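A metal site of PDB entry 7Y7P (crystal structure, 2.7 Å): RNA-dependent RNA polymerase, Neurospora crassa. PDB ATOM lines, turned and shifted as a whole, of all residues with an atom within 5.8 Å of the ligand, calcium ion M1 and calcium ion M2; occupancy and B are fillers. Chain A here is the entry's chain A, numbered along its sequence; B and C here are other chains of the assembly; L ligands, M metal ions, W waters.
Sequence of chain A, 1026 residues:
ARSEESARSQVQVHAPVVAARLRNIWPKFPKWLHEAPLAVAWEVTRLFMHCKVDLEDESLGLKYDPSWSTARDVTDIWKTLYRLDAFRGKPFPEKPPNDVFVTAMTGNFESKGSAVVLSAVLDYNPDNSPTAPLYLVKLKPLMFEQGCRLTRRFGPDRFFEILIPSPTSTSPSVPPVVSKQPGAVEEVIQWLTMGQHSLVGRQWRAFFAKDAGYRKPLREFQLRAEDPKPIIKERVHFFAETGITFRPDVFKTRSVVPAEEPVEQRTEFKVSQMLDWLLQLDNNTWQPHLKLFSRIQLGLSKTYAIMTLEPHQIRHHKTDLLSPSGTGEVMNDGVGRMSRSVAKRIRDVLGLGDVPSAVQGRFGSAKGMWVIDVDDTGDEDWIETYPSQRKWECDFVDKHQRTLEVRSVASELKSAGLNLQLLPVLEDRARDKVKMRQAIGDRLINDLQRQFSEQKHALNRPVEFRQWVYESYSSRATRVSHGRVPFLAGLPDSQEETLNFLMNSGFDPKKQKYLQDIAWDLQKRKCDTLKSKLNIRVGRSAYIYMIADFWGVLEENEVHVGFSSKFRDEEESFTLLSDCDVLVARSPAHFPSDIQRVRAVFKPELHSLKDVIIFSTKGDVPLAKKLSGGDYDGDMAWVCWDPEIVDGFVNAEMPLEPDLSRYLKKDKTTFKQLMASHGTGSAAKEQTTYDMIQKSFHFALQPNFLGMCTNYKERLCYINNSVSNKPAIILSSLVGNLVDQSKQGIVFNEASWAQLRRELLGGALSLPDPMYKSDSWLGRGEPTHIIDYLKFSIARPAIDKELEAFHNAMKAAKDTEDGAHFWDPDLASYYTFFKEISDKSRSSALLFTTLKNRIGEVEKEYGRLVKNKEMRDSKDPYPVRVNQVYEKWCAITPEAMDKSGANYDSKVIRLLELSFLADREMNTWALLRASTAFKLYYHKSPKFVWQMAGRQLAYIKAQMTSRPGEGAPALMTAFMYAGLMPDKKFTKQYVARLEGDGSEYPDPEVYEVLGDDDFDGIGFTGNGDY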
ATOM      1  N   ARG A 295     -13.947  -4.579 -23.130  1.00  0.00           N
ATOM      2  CA  ARG A 295     -13.607  -5.818 -22.413  1.00  0.00           C
ATOM      3  C   ARG A 295     -12.646  -6.703 -23.223  1.00  0.00           C
ATOM      4  O   ARG A 295     -12.218  -7.728 -22.674  1.00  0.00           O
ATOM      5  CB  ARG A 295     -14.887  -6.535 -21.995  1.00  0.00           C
ATOM      6  CG  ARG A 295     -15.890  -5.648 -21.260  1.00  0.00           C
ATOM      7  CD  ARG A 295     -15.261  -4.951 -20.088  1.00  0.00           C
ATOM      8  NE  ARG A 295     -16.245  -4.189 -19.349  1.00  0.00           N
ATOM      9  CZ  ARG A 295     -15.981  -3.492 -18.256  1.00  0.00           C
ATOM     10  NH1 ARG A 295     -14.753  -3.463 -17.782  1.00  0.00           N
ATOM     11  NH2 ARG A 295     -16.949  -2.829 -17.645  1.00  0.00           N
ATOM     12  N   ASP A 333     -16.963  -4.184  -4.285  1.00  0.00           N
ATOM     13  CA  ASP A 333     -16.783  -4.017  -5.725  1.00  0.00           C
ATOM     14  C   ASP A 333     -15.461  -4.590  -6.224  1.00  0.00           C
ATOM     15  O   ASP A 333     -14.397  -4.016  -5.988  1.00  0.00           O
ATOM     16  CB  ASP A 333     -16.887  -2.533  -6.101  1.00  0.00           C
ATOM     17  CG  ASP A 333     -17.125  -2.330  -7.575  1.00  0.00           C
ATOM     18  OD1 ASP A 333     -17.140  -3.332  -8.319  1.00  0.00           O
ATOM     19  OD2 ASP A 333     -17.306  -1.168  -8.002  1.00  0.00           O
ATOM     20  N   LYS A 367     -13.053  -9.798 -13.236  1.00  0.00           N
ATOM     21  CA  LYS A 367     -11.853  -8.983 -13.106  1.00  0.00           C
ATOM     22  C   LYS A 367     -11.801  -8.389 -11.706  1.00  0.00           C
ATOM     23  O   LYS A 367     -12.830  -7.936 -11.187  1.00  0.00           O
ATOM     24  CB  LYS A 367     -11.814  -7.867 -14.162  1.00  0.00           C
ATOM     25  CG  LYS A 367     -10.537  -7.024 -14.142  1.00  0.00           C
ATOM     26  CD  LYS A 367     -10.727  -5.684 -14.846  1.00  0.00           C
ATOM     27  CE  LYS A 367     -12.010  -5.007 -14.411  1.00  0.00           C
ATOM     28  NZ  LYS A 367     -11.788  -4.074 -13.270  1.00  0.00           N
ATOM     29  N   SER A 388     -20.155  -7.581  -9.312  1.00  0.00           N
ATOM     30  CA  SER A 388     -19.240  -6.463  -9.536  1.00  0.00           C
ATOM     31  C   SER A 388     -17.970  -6.889 -10.262  1.00  0.00           C
ATOM     32  O   SER A 388     -17.317  -6.041 -10.891  1.00  0.00           O
ATOM     33  CB  SER A 388     -18.876  -5.814  -8.196  1.00  0.00           C
ATOM     34  OG  SER A 388     -18.309  -6.753  -7.303  1.00  0.00           O
ATOM     35  N   LYS A 391     -17.561  -8.977 -15.868  1.00  0.00           N
ATOM     36  CA  LYS A 391     -17.770  -7.888 -16.811  1.00  0.00           C
ATOM     37  C   LYS A 391     -18.671  -8.278 -17.983  1.00  0.00           C
ATOM     38  O   LYS A 391     -19.142  -7.383 -18.700  1.00  0.00           O
ATOM     39  CB  LYS A 391     -16.425  -7.379 -17.341  1.00  0.00           C
ATOM     40  CG  LYS A 391     -15.549  -6.781 -16.251  1.00  0.00           C
ATOM     41  CD  LYS A 391     -16.329  -5.810 -15.391  1.00  0.00           C
ATOM     42  CE  LYS A 391     -15.580  -5.474 -14.115  1.00  0.00           C
ATOM     43  NZ  LYS A 391     -16.373  -4.577 -13.230  1.00  0.00           N
ATOM     44  N   ARG A 586      -6.216   8.095  -2.877  1.00  0.00           N
ATOM     45  CA  ARG A 586      -5.913   7.375  -4.121  1.00  0.00           C
ATOM     46  C   ARG A 586      -5.601   8.416  -5.194  1.00  0.00           C
ATOM     47  O   ARG A 586      -6.029   9.556  -5.032  1.00  0.00           O
ATOM     48  CB  ARG A 586      -7.119   6.510  -4.504  1.00  0.00           C
ATOM     49  CG  ARG A 586      -6.786   5.264  -5.301  1.00  0.00           C
ATOM     50  CD  ARG A 586      -8.041   4.454  -5.572  1.00  0.00           C
ATOM     51  NE  ARG A 586      -8.912   5.043  -6.570  1.00  0.00           N
ATOM     52  CZ  ARG A 586      -8.767   4.915  -7.881  1.00  0.00           C
ATOM     53  NH1 ARG A 586      -7.775   4.206  -8.385  1.00  0.00           N
ATOM     54  NH2 ARG A 586      -9.628   5.500  -8.697  1.00  0.00           N
ATOM     55  N   SER A 587      -4.846   8.033  -6.213  1.00  0.00           N
ATOM     56  CA  SER A 587      -4.579   8.945  -7.355  1.00  0.00           C
ATOM     57  C   SER A 587      -5.435   8.462  -8.521  1.00  0.00           C
ATOM     58  O   SER A 587      -5.582   7.241  -8.657  1.00  0.00           O
ATOM     59  CB  SER A 587      -3.124   8.932  -7.703  1.00  0.00           C
ATOM     60  OG  SER A 587      -2.916   9.544  -8.966  1.00  0.00           O
ATOM     61  N   PRO A 588      -6.033   9.341  -9.361  1.00  0.00           N
ATOM     62  CA  PRO A 588      -5.900  10.788  -9.227  1.00  0.00           C
ATOM     63  C   PRO A 588      -6.732  11.364  -8.077  1.00  0.00           C
ATOM     64  O   PRO A 588      -7.838  10.923  -7.885  1.00  0.00           O
ATOM     65  CB  PRO A 588      -6.434  11.318 -10.561  1.00  0.00           C
ATOM     66  CG  PRO A 588      -6.507  10.122 -11.453  1.00  0.00           C
ATOM     67  CD  PRO A 588      -6.840   8.980 -10.512  1.00  0.00           C
ATOM     68  N   SER A 628     -11.838   8.791  -4.844  1.00  0.00           N
ATOM     69  CA  SER A 628     -11.862   8.959  -6.320  1.00  0.00           C
ATOM     70  C   SER A 628     -12.638   7.865  -7.044  1.00  0.00           C
ATOM     71  O   SER A 628     -12.209   7.475  -8.132  1.00  0.00           O
ATOM     72  CB  SER A 628     -10.482   9.130  -6.883  1.00  0.00           C
ATOM     73  OG  SER A 628     -10.502   9.925  -8.057  1.00  0.00           O
ATOM     74  N   GLY A 629     -13.792   7.453  -6.508  1.00  0.00           N
ATOM     75  CA  GLY A 629     -14.586   6.374  -7.121  1.00  0.00           C
ATOM     76  C   GLY A 629     -13.830   5.072  -7.194  1.00  0.00           C
ATOM     77  O   GLY A 629     -13.924   4.388  -8.230  1.00  0.00           O
ATOM     78  N   GLY A 630     -13.114   4.758  -6.128  1.00  0.00           N
ATOM     79  CA  GLY A 630     -12.266   3.554  -6.107  1.00  0.00           C
ATOM     80  C   GLY A 630     -12.997   2.271  -5.847  1.00  0.00           C
ATOM     81  O   GLY A 630     -14.141   2.320  -5.375  1.00  0.00           O
ATOM     82  N   ASP A 631     -12.317   1.154  -6.093  1.00  0.00           N
ATOM     83  CA  ASP A 631     -12.930  -0.176  -5.907  1.00  0.00           C
ATOM     84  C   ASP A 631     -11.899  -1.114  -5.292  1.00  0.00           C
ATOM     85  O   ASP A 631     -10.845  -0.651  -4.878  1.00  0.00           O
ATOM     86  CB  ASP A 631     -13.537  -0.745  -7.195  1.00  0.00           C
ATOM     87  CG  ASP A 631     -12.762  -0.555  -8.472  1.00  0.00           C
ATOM     88  OD1 ASP A 631     -11.579  -0.248  -8.391  1.00  0.00           O
ATOM     89  OD2 ASP A 631     -13.367  -0.722  -9.545  1.00  0.00           O
ATOM     90  N   TYR A 632     -12.253  -2.388  -5.179  1.00  0.00           N
ATOM     91  CA  TYR A 632     -11.335  -3.416  -4.635  1.00  0.00           C
ATOM     92  C   TYR A 632     -10.956  -4.359  -5.787  1.00  0.00           C
ATOM     93  O   TYR A 632     -10.912  -5.555  -5.563  1.00  0.00           O
ATOM     94  CB  TYR A 632     -11.987  -4.073  -3.425  1.00  0.00           C
ATOM     95  CG  TYR A 632     -12.581  -3.101  -2.436  1.00  0.00           C
ATOM     96  CD1 TYR A 632     -11.787  -2.496  -1.473  1.00  0.00           C
ATOM     97  CD2 TYR A 632     -13.925  -2.792  -2.448  1.00  0.00           C
ATOM     98  CE1 TYR A 632     -12.311  -1.609  -0.557  1.00  0.00           C
ATOM     99  CE2 TYR A 632     -14.471  -1.899  -1.551  1.00  0.00           C
ATOM    100  CZ  TYR A 632     -13.667  -1.317  -0.590  1.00  0.00           C
ATOM    101  OH  TYR A 632     -14.189  -0.428   0.309  1.00  0.00           O
ATOM    102  N   ASP A 633     -10.765  -3.824  -6.991  1.00  0.00           N
ATOM    103  CA  ASP A 633     -10.479  -4.623  -8.218  1.00  0.00           C
ATOM    104  C   ASP A 633      -9.011  -4.553  -8.653  1.00  0.00           C
ATOM    105  O   ASP A 633      -8.716  -4.979  -9.773  1.00  0.00           O
ATOM    106  CB  ASP A 633     -11.428  -4.207  -9.341  1.00  0.00           C
ATOM    107  CG  ASP A 633     -11.081  -2.937 -10.082  1.00  0.00           C
ATOM    108  OD1 ASP A 633     -10.178  -2.198  -9.657  1.00  0.00           O
ATOM    109  OD2 ASP A 633     -11.754  -2.681 -11.086  1.00  0.00           O
ATOM    110  N   GLY A 634      -8.109  -4.091  -7.795  1.00  0.00           N
ATOM    111  CA  GLY A 634      -6.707  -3.884  -8.174  1.00  0.00           C
ATOM    112  C   GLY A 634      -6.260  -2.520  -7.737  1.00  0.00           C
ATOM    113  O   GLY A 634      -5.086  -2.187  -7.940  1.00  0.00           O
ATOM    114  N   ASP A 635      -7.181  -1.763  -7.173  1.00  0.00           N
ATOM    115  CA  ASP A 635      -6.881  -0.401  -6.689  1.00  0.00           C
ATOM    116  C   ASP A 635      -5.887  -0.434  -5.518  1.00  0.00           C
ATOM    117  O   ASP A 635      -5.956  -1.366  -4.718  1.00  0.00           O
ATOM    118  CB  ASP A 635      -8.149   0.296  -6.209  1.00  0.00           C
ATOM    119  CG  ASP A 635      -8.988   0.890  -7.314  1.00  0.00           C
ATOM    120  OD1 ASP A 635      -8.956   0.344  -8.422  1.00  0.00           O
ATOM    121  OD2 ASP A 635      -9.668   1.880  -7.036  1.00  0.00           O
ATOM    122  N   LEU A 706      -8.355  14.671 -21.458  1.00  0.00           N
ATOM    123  CA  LEU A 706      -8.138  14.452 -20.001  1.00  0.00           C
ATOM    124  C   LEU A 706      -6.914  15.249 -19.559  1.00  0.00           C
ATOM    125  O   LEU A 706      -7.008  15.922 -18.530  1.00  0.00           O
ATOM    126  CB  LEU A 706      -7.912  12.960 -19.734  1.00  0.00           C
ATOM    127  CG  LEU A 706      -7.375  12.610 -18.347  1.00  0.00           C
ATOM    128  CD1 LEU A 706      -8.454  12.771 -17.297  1.00  0.00           C
ATOM    129  CD2 LEU A 706      -6.827  11.192 -18.331  1.00  0.00           C
ATOM    130  N   GLY A 736     -12.882  13.451 -13.806  1.00  0.00           N
ATOM    131  CA  GLY A 736     -13.333  12.131 -13.330  1.00  0.00           C
ATOM    132  C   GLY A 736     -14.128  11.395 -14.386  1.00  0.00           C
ATOM    133  O   GLY A 736     -14.028  10.182 -14.451  1.00  0.00           O
ATOM    134  N   VAL A 739     -11.654  10.300 -17.666  1.00  0.00           N
ATOM    135  CA  VAL A 739     -10.742   9.127 -17.469  1.00  0.00           C
ATOM    136  C   VAL A 739     -11.516   7.851 -17.782  1.00  0.00           C
ATOM    137  O   VAL A 739     -10.899   6.901 -18.279  1.00  0.00           O
ATOM    138  CB  VAL A 739     -10.098   9.135 -16.066  1.00  0.00           C
ATOM    139  CG1 VAL A 739     -11.105   9.010 -14.943  1.00  0.00           C
ATOM    140  CG2 VAL A 739      -8.998   8.099 -15.935  1.00  0.00           C
ATOM    141  N   ASP A 740     -12.823   7.846 -17.536  1.00  0.00           N
ATOM    142  CA  ASP A 740     -13.669   6.653 -17.759  1.00  0.00           C
ATOM    143  C   ASP A 740     -14.345   6.745 -19.124  1.00  0.00           C
ATOM    144  O   ASP A 740     -15.344   6.049 -19.315  1.00  0.00           O
ATOM    145  CB  ASP A 740     -14.705   6.548 -16.649  1.00  0.00           C
ATOM    146  CG  ASP A 740     -14.121   6.594 -15.254  1.00  0.00           C
ATOM    147  OD1 ASP A 740     -12.986   6.124 -15.089  1.00  0.00           O
ATOM    148  OD2 ASP A 740     -14.808   7.085 -14.349  1.00  0.00           O
ATOM    149  N   LYS A 743     -14.821   3.254 -21.345  1.00  0.00           N
ATOM    150  CA  LYS A 743     -15.842   2.345 -20.774  1.00  0.00           C
ATOM    151  C   LYS A 743     -17.222   3.001 -20.758  1.00  0.00           C
ATOM    152  O   LYS A 743     -18.207   2.288 -20.943  1.00  0.00           O
ATOM    153  CB  LYS A 743     -15.402   1.822 -19.404  1.00  0.00           C
ATOM    154  CG  LYS A 743     -14.977   0.361 -19.378  1.00  0.00           C
ATOM    155  CD  LYS A 743     -14.031   0.046 -18.249  1.00  0.00           C
ATOM    156  CE  LYS A 743     -12.651  -0.358 -18.720  1.00  0.00           C
ATOM    157  NZ  LYS A 743     -11.718  -0.529 -17.586  1.00  0.00           N
ATOM    158  P     C B   7      -6.529  -2.885 -14.585  1.00  0.00           P
ATOM    159  OP1   C B   7      -7.613  -3.787 -14.108  1.00  0.00           O
ATOM    160  OP2   C B   7      -6.604  -2.295 -15.943  1.00  0.00           O
ATOM    161  O5'   C B   7      -6.408  -1.704 -13.525  1.00  0.00           O
ATOM    162  C5'   C B   7      -6.336  -1.974 -12.138  1.00  0.00           C
ATOM    163  C4'   C B   7      -6.499  -0.716 -11.324  1.00  0.00           C
ATOM    164  O4'   C B   7      -5.256   0.035 -11.338  1.00  0.00           O
ATOM    165  C3'   C B   7      -7.533   0.267 -11.847  1.00  0.00           C
ATOM    166  O3'   C B   7      -8.857  -0.071 -11.481  1.00  0.00           O
ATOM    167  C2'   C B   7      -7.059   1.591 -11.253  1.00  0.00           C
ATOM    168  O2'   C B   7      -7.426   1.689  -9.885  1.00  0.00           O
ATOM    169  C1'   C B   7      -5.538   1.416 -11.327  1.00  0.00           C
ATOM    170  N1    C B   7      -4.958   2.013 -12.559  1.00  0.00           N
ATOM    171  C2    C B   7      -4.587   3.360 -12.543  1.00  0.00           C
ATOM    172  O2    C B   7      -4.746   4.018 -11.507  1.00  0.00           O
ATOM    173  N3    C B   7      -4.062   3.913 -13.665  1.00  0.00           N
ATOM    174  C4    C B   7      -3.901   3.163 -14.771  1.00  0.00           C
ATOM    175  N4    C B   7      -3.384   3.754 -15.848  1.00  0.00           N
ATOM    176  C5    C B   7      -4.283   1.791 -14.803  1.00  0.00           C
ATOM    177  C6    C B   7      -4.800   1.260 -13.689  1.00  0.00           C
ATOM    178  P     U C   7      -0.520  14.995 -20.748  1.00  0.00           P
ATOM    179  OP1   U C   7       0.703  15.814 -20.720  1.00  0.00           O
ATOM    180  OP2   U C   7      -0.513  13.678 -21.423  1.00  0.00           O
ATOM    181  O5'   U C   7      -1.029  14.798 -19.258  1.00  0.00           O
ATOM    182  C5'   U C   7      -1.158  15.906 -18.372  1.00  0.00           C
ATOM    183  C4'   U C   7      -1.762  15.453 -17.072  1.00  0.00           C
ATOM    184  O4'   U C   7      -2.996  14.740 -17.334  1.00  0.00           O
ATOM    185  C3'   U C   7      -0.942  14.444 -16.274  1.00  0.00           C
ATOM    186  O3'   U C   7       0.109  15.016 -15.507  1.00  0.00           O
ATOM    187  C2'   U C   7      -2.014  13.836 -15.390  1.00  0.00           C
ATOM    188  O2'   U C   7      -2.377  14.682 -14.325  1.00  0.00           O
ATOM    189  C1'   U C   7      -3.182  13.719 -16.366  1.00  0.00           C
ATOM    190  N1    U C   7      -3.227  12.426 -17.056  1.00  0.00           N
ATOM    191  C2    U C   7      -3.667  11.336 -16.332  1.00  0.00           C
ATOM    192  O2    U C   7      -4.049  11.408 -15.174  1.00  0.00           O
ATOM    193  N3    U C   7      -3.672  10.153 -17.021  1.00  0.00           N
ATOM    194  C4    U C   7      -3.286   9.943 -18.326  1.00  0.00           C
ATOM    195  O4    U C   7      -3.358   8.819 -18.810  1.00  0.00           O
ATOM    196  C5    U C   7      -2.827  11.118 -19.001  1.00  0.00           C
ATOM    197  C6    U C   7      -2.817  12.293 -18.365  1.00  0.00           C
ATOM    198  P     G C   8       1.403  14.154 -15.207  1.00  0.00           P
ATOM    199  OP1   G C   8       2.559  15.080 -14.899  1.00  0.00           O
ATOM    200  OP2   G C   8       1.638  13.199 -16.348  1.00  0.00           O
ATOM    201  O5'   G C   8       1.026  13.338 -13.879  1.00  0.00           O
ATOM    202  C5'   G C   8       0.790  14.074 -12.660  1.00  0.00           C
ATOM    203  C4'   G C   8      -0.028  13.230 -11.710  1.00  0.00           C
ATOM    204  O4'   G C   8      -1.200  12.712 -12.392  1.00  0.00           O
ATOM    205  C3'   G C   8       0.650  11.961 -11.185  1.00  0.00           C
ATOM    206  O3'   G C   8       1.593  12.228 -10.153  1.00  0.00           O
ATOM    207  C2'   G C   8      -0.582  11.180 -10.717  1.00  0.00           C
ATOM    208  O2'   G C   8      -1.097  11.671  -9.504  1.00  0.00           O
ATOM    209  C1'   G C   8      -1.535  11.451 -11.876  1.00  0.00           C
ATOM    210  N9    G C   8      -1.445  10.460 -12.945  1.00  0.00           N
ATOM    211  C8    G C   8      -0.825  10.624 -14.151  1.00  0.00           C
ATOM    212  N7    G C   8      -0.902   9.555 -14.916  1.00  0.00           N
ATOM    213  C5    G C   8      -1.614   8.646 -14.162  1.00  0.00           C
ATOM    214  C6    G C   8      -2.002   7.314 -14.476  1.00  0.00           C
ATOM    215  O6    G C   8      -1.783   6.677 -15.509  1.00  0.00           O
ATOM    216  N1    G C   8      -2.714   6.737 -13.421  1.00  0.00           N
ATOM    217  C2    G C   8      -3.010   7.349 -12.237  1.00  0.00           C
ATOM    218  N2    G C   8      -3.708   6.635 -11.350  1.00  0.00           N
ATOM    219  N3    G C   8      -2.657   8.600 -11.937  1.00  0.00           N
ATOM    220  C4    G C   8      -1.953   9.179 -12.946  1.00  0.00           C
HETATM  221  P1  LIG L   1     -11.343   0.745 -13.236  1.00  0.00           P
HETATM  222  P2  LIG L   1     -14.085   0.950 -13.857  1.00  0.00           P
HETATM  223  P3  LIG L   1     -14.774  -1.699 -14.661  1.00  0.00           P
HETATM  224  O1  LIG L   1     -10.059   0.532 -13.999  1.00  0.00           O
HETATM  225  O2  LIG L   1     -14.474   2.330 -14.305  1.00  0.00           O
HETATM  226  O3  LIG L   1     -13.717  -2.050 -15.674  1.00  0.00           O
HETATM  227  O4  LIG L   1     -11.687  -0.139 -12.071  1.00  0.00           O
HETATM  228  O5  LIG L   1     -14.247   0.564 -12.408  1.00  0.00           O
HETATM  229  O6  LIG L   1     -16.164  -2.188 -14.996  1.00  0.00           O
HETATM  230  N1  LIG L   1     -12.559   0.712 -14.307  1.00  0.00           N
HETATM  231  O7  LIG L   1     -14.890  -0.095 -14.801  1.00  0.00           O
HETATM  232  O8  LIG L   1     -14.381  -1.958 -13.234  1.00  0.00           O
HETATM  233  O9  LIG L   1     -11.390   2.281 -12.755  1.00  0.00           O
HETATM  234  C1  LIG L   1     -10.507   3.232 -13.349  1.00  0.00           C
HETATM  235  C2  LIG L   1     -10.168   4.335 -12.343  1.00  0.00           C
HETATM  236  O10 LIG L   1      -8.787   4.247 -11.994  1.00  0.00           O
HETATM  237  C3  LIG L   1     -10.385   5.713 -12.934  1.00  0.00           C
HETATM  238  O11 LIG L   1     -11.651   6.249 -12.538  1.00  0.00           O
HETATM  239  C4  LIG L   1      -9.245   6.522 -12.354  1.00  0.00           C
HETATM  240  O12 LIG L   1      -9.595   7.055 -11.075  1.00  0.00           O
HETATM  241  C5  LIG L   1      -8.134   5.501 -12.185  1.00  0.00           C
HETATM  242  N2  LIG L   1      -7.415   5.456 -13.481  1.00  0.00           N
HETATM  243  C6  LIG L   1      -7.449   4.416 -14.338  1.00  0.00           C
HETATM  244  N3  LIG L   1      -6.683   4.668 -15.433  1.00  0.00           N
HETATM  245  C7  LIG L   1      -6.164   5.898 -15.285  1.00  0.00           C
HETATM  246  C8  LIG L   1      -5.283   6.770 -16.083  1.00  0.00           C
HETATM  247  N4  LIG L   1      -4.790   6.366 -17.282  1.00  0.00           N
HETATM  248  N5  LIG L   1      -4.974   7.983 -15.570  1.00  0.00           N
HETATM  249  C9  LIG L   1      -5.449   8.386 -14.381  1.00  0.00           C
HETATM  250  N6  LIG L   1      -6.267   7.653 -13.605  1.00  0.00           N
HETATM  251  C10 LIG L   1      -6.647   6.410 -13.995  1.00  0.00           C
HETATM  252 CA    CA M   1     -10.579   0.049 -10.014  1.00  0.00          CA
HETATM  253 CA    CA M   2     -13.865  -1.266 -11.256  1.00  0.00          CA
HETATM  254 CA    CA M   3     -14.621   3.718 -10.555  1.00  0.00          CA
HETATM  255  O   HOH W   1     -16.368  -0.968 -10.612  1.00  0.00           O
HETATM  256  O   HOH W   2     -11.145   2.187  -9.057  1.00  0.00           O
HETATM  257  O   HOH W   3      -6.234   3.770 -17.736  1.00  0.00           O
HETATM  258  O   HOH W   4     -15.135  -3.061  -9.842  1.00  0.00           O
HETATM  259  O   HOH W   5     -14.208   5.105 -12.587  1.00  0.00           O
HETATM  260  O   HOH W   6     -12.588   5.896 -10.117  1.00  0.00           O
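N4 of C 7 of chain B sits at hydrogen-bond distance from a nitrogen (N4) of the ligand, 3.3 Å away. O4 of U 7 of chain C sits at hydrogen-bond distance from a nitrogen (N4) of the ligand (3.2 Å). NH1 of Arg 295 lies within salt-bridge range of O3 of the ligand (2.7 Å). NH2 of Arg 586 lies within hydrogen-bond range of O12 of the ligand (2.8 Å). NZ of Lys 367 is in salt-bridge range of O3 of the ligand, 3.7 Å away. OD1 of Asp 740 is in hydrogen-bond range of O11 of the ligand (2.9 Å). An oxygen (O3) of the ligand lies within salt-bridge range of the side-chain amino group (NZ) of Lys 743 (3.2 Å). O6 of the ligand is in salt-bridge range of NZ of Lys 391 (3.0 Å).
OG of Ser 587 lies within hydrogen-bond range of O2' of G 8 of chain C (2.8 Å). OD2 of Asp 635 is in salt-bridge range of NE of Arg 586 (3.3 Å). The side-chain amino group of Lys 391 lies within hydrogen-bond range of the backbone carbonyl oxygen of Ser 388, at 2.9 Å. OD2 of Asp 633 sits close to NZ of Lys 367 (2.6 Å). NH2 of Arg 586 lies within hydrogen-bond range of O of Ser 628. O2' of C 7 of chain B is in hydrogen-bond range of the guanidinium group of Arg 586. The backbone carbonyl oxygen (O) of Pro 588 sits at hydrogen-bond distance from the side-chain hydroxyl (OG) of Ser 628, 2.8 Å away.
N5 of the ligand sits close to N1 of G 8 of chain C (3.4 Å). Residues that only touch the ligand: Pro 588, Ser 628 and Val 739. Hydrophobic or aromatic side chains within 4 Å of the ligand: Pro 588 and Val 739. Within 4 Å of the ligand: Arg 295, Lys 367, Lys 391, Arg 586, Pro 588, Ser 628, Asp 631, Asp 633, Val 739, Asp 740, Lys 743, C 7 of chain B, U 7 of chain C and G 8 of chain C.
Four residues have an atom within 4 Å of calcium ion M1: Asp 631, Asp 633, Asp 635 and C 7 of chain B.
Of the 24 residues printed, 2 come within 4 Å of calcium ion M2. The nearest printed residue that does not touch calcium ion M2 is Lys 367 (4.03 Å).
Calcium ion M1 is bound by the side-chain carboxylate of Asp 631 (1.9 Å), O3' of C 7 of chain B (2.3 Å), the side-chain carboxylate of Asp 635 (2.3 Å), the side-chain carboxylate of Asp 633 (2.3 Å), an oxygen (O4) of the ligand (2.3 Å) and water W2 (2.4 Å). Calcium ion M1 has six donor atoms within binding distance. Slightly farther from calcium ion M1 lies the side-chain carboxylate (OD2) of Asp 631 (2.9 Å).
Calcium ion M2 is bound by OD2 of Asp 631, O8 of the ligand, O5 of the ligand, OD2 of Asp 633, O4 of the ligand, water W1 and water W4. Calcium ion M2 has seven donor atoms within binding distance.
Water W2 bridges OD2 of Asp 635 (2.5 Å) and N of Asp 631 (3.4 Å). Water W3 bridges a nitrogen (N3) of the ligand (2.5 Å) and N4 of C 7 of chain B (3.4 Å). Water W6 lies within hydrogen-bond range of O of Ser 628 (2.6 Å), O11 of the ligand (2.6 Å) and NH2 of Arg 586 (3.3 Å). Water W5 bridges the side-chain carboxylate (OD2) of Asp 740 and an oxygen (O11) of the ligand.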
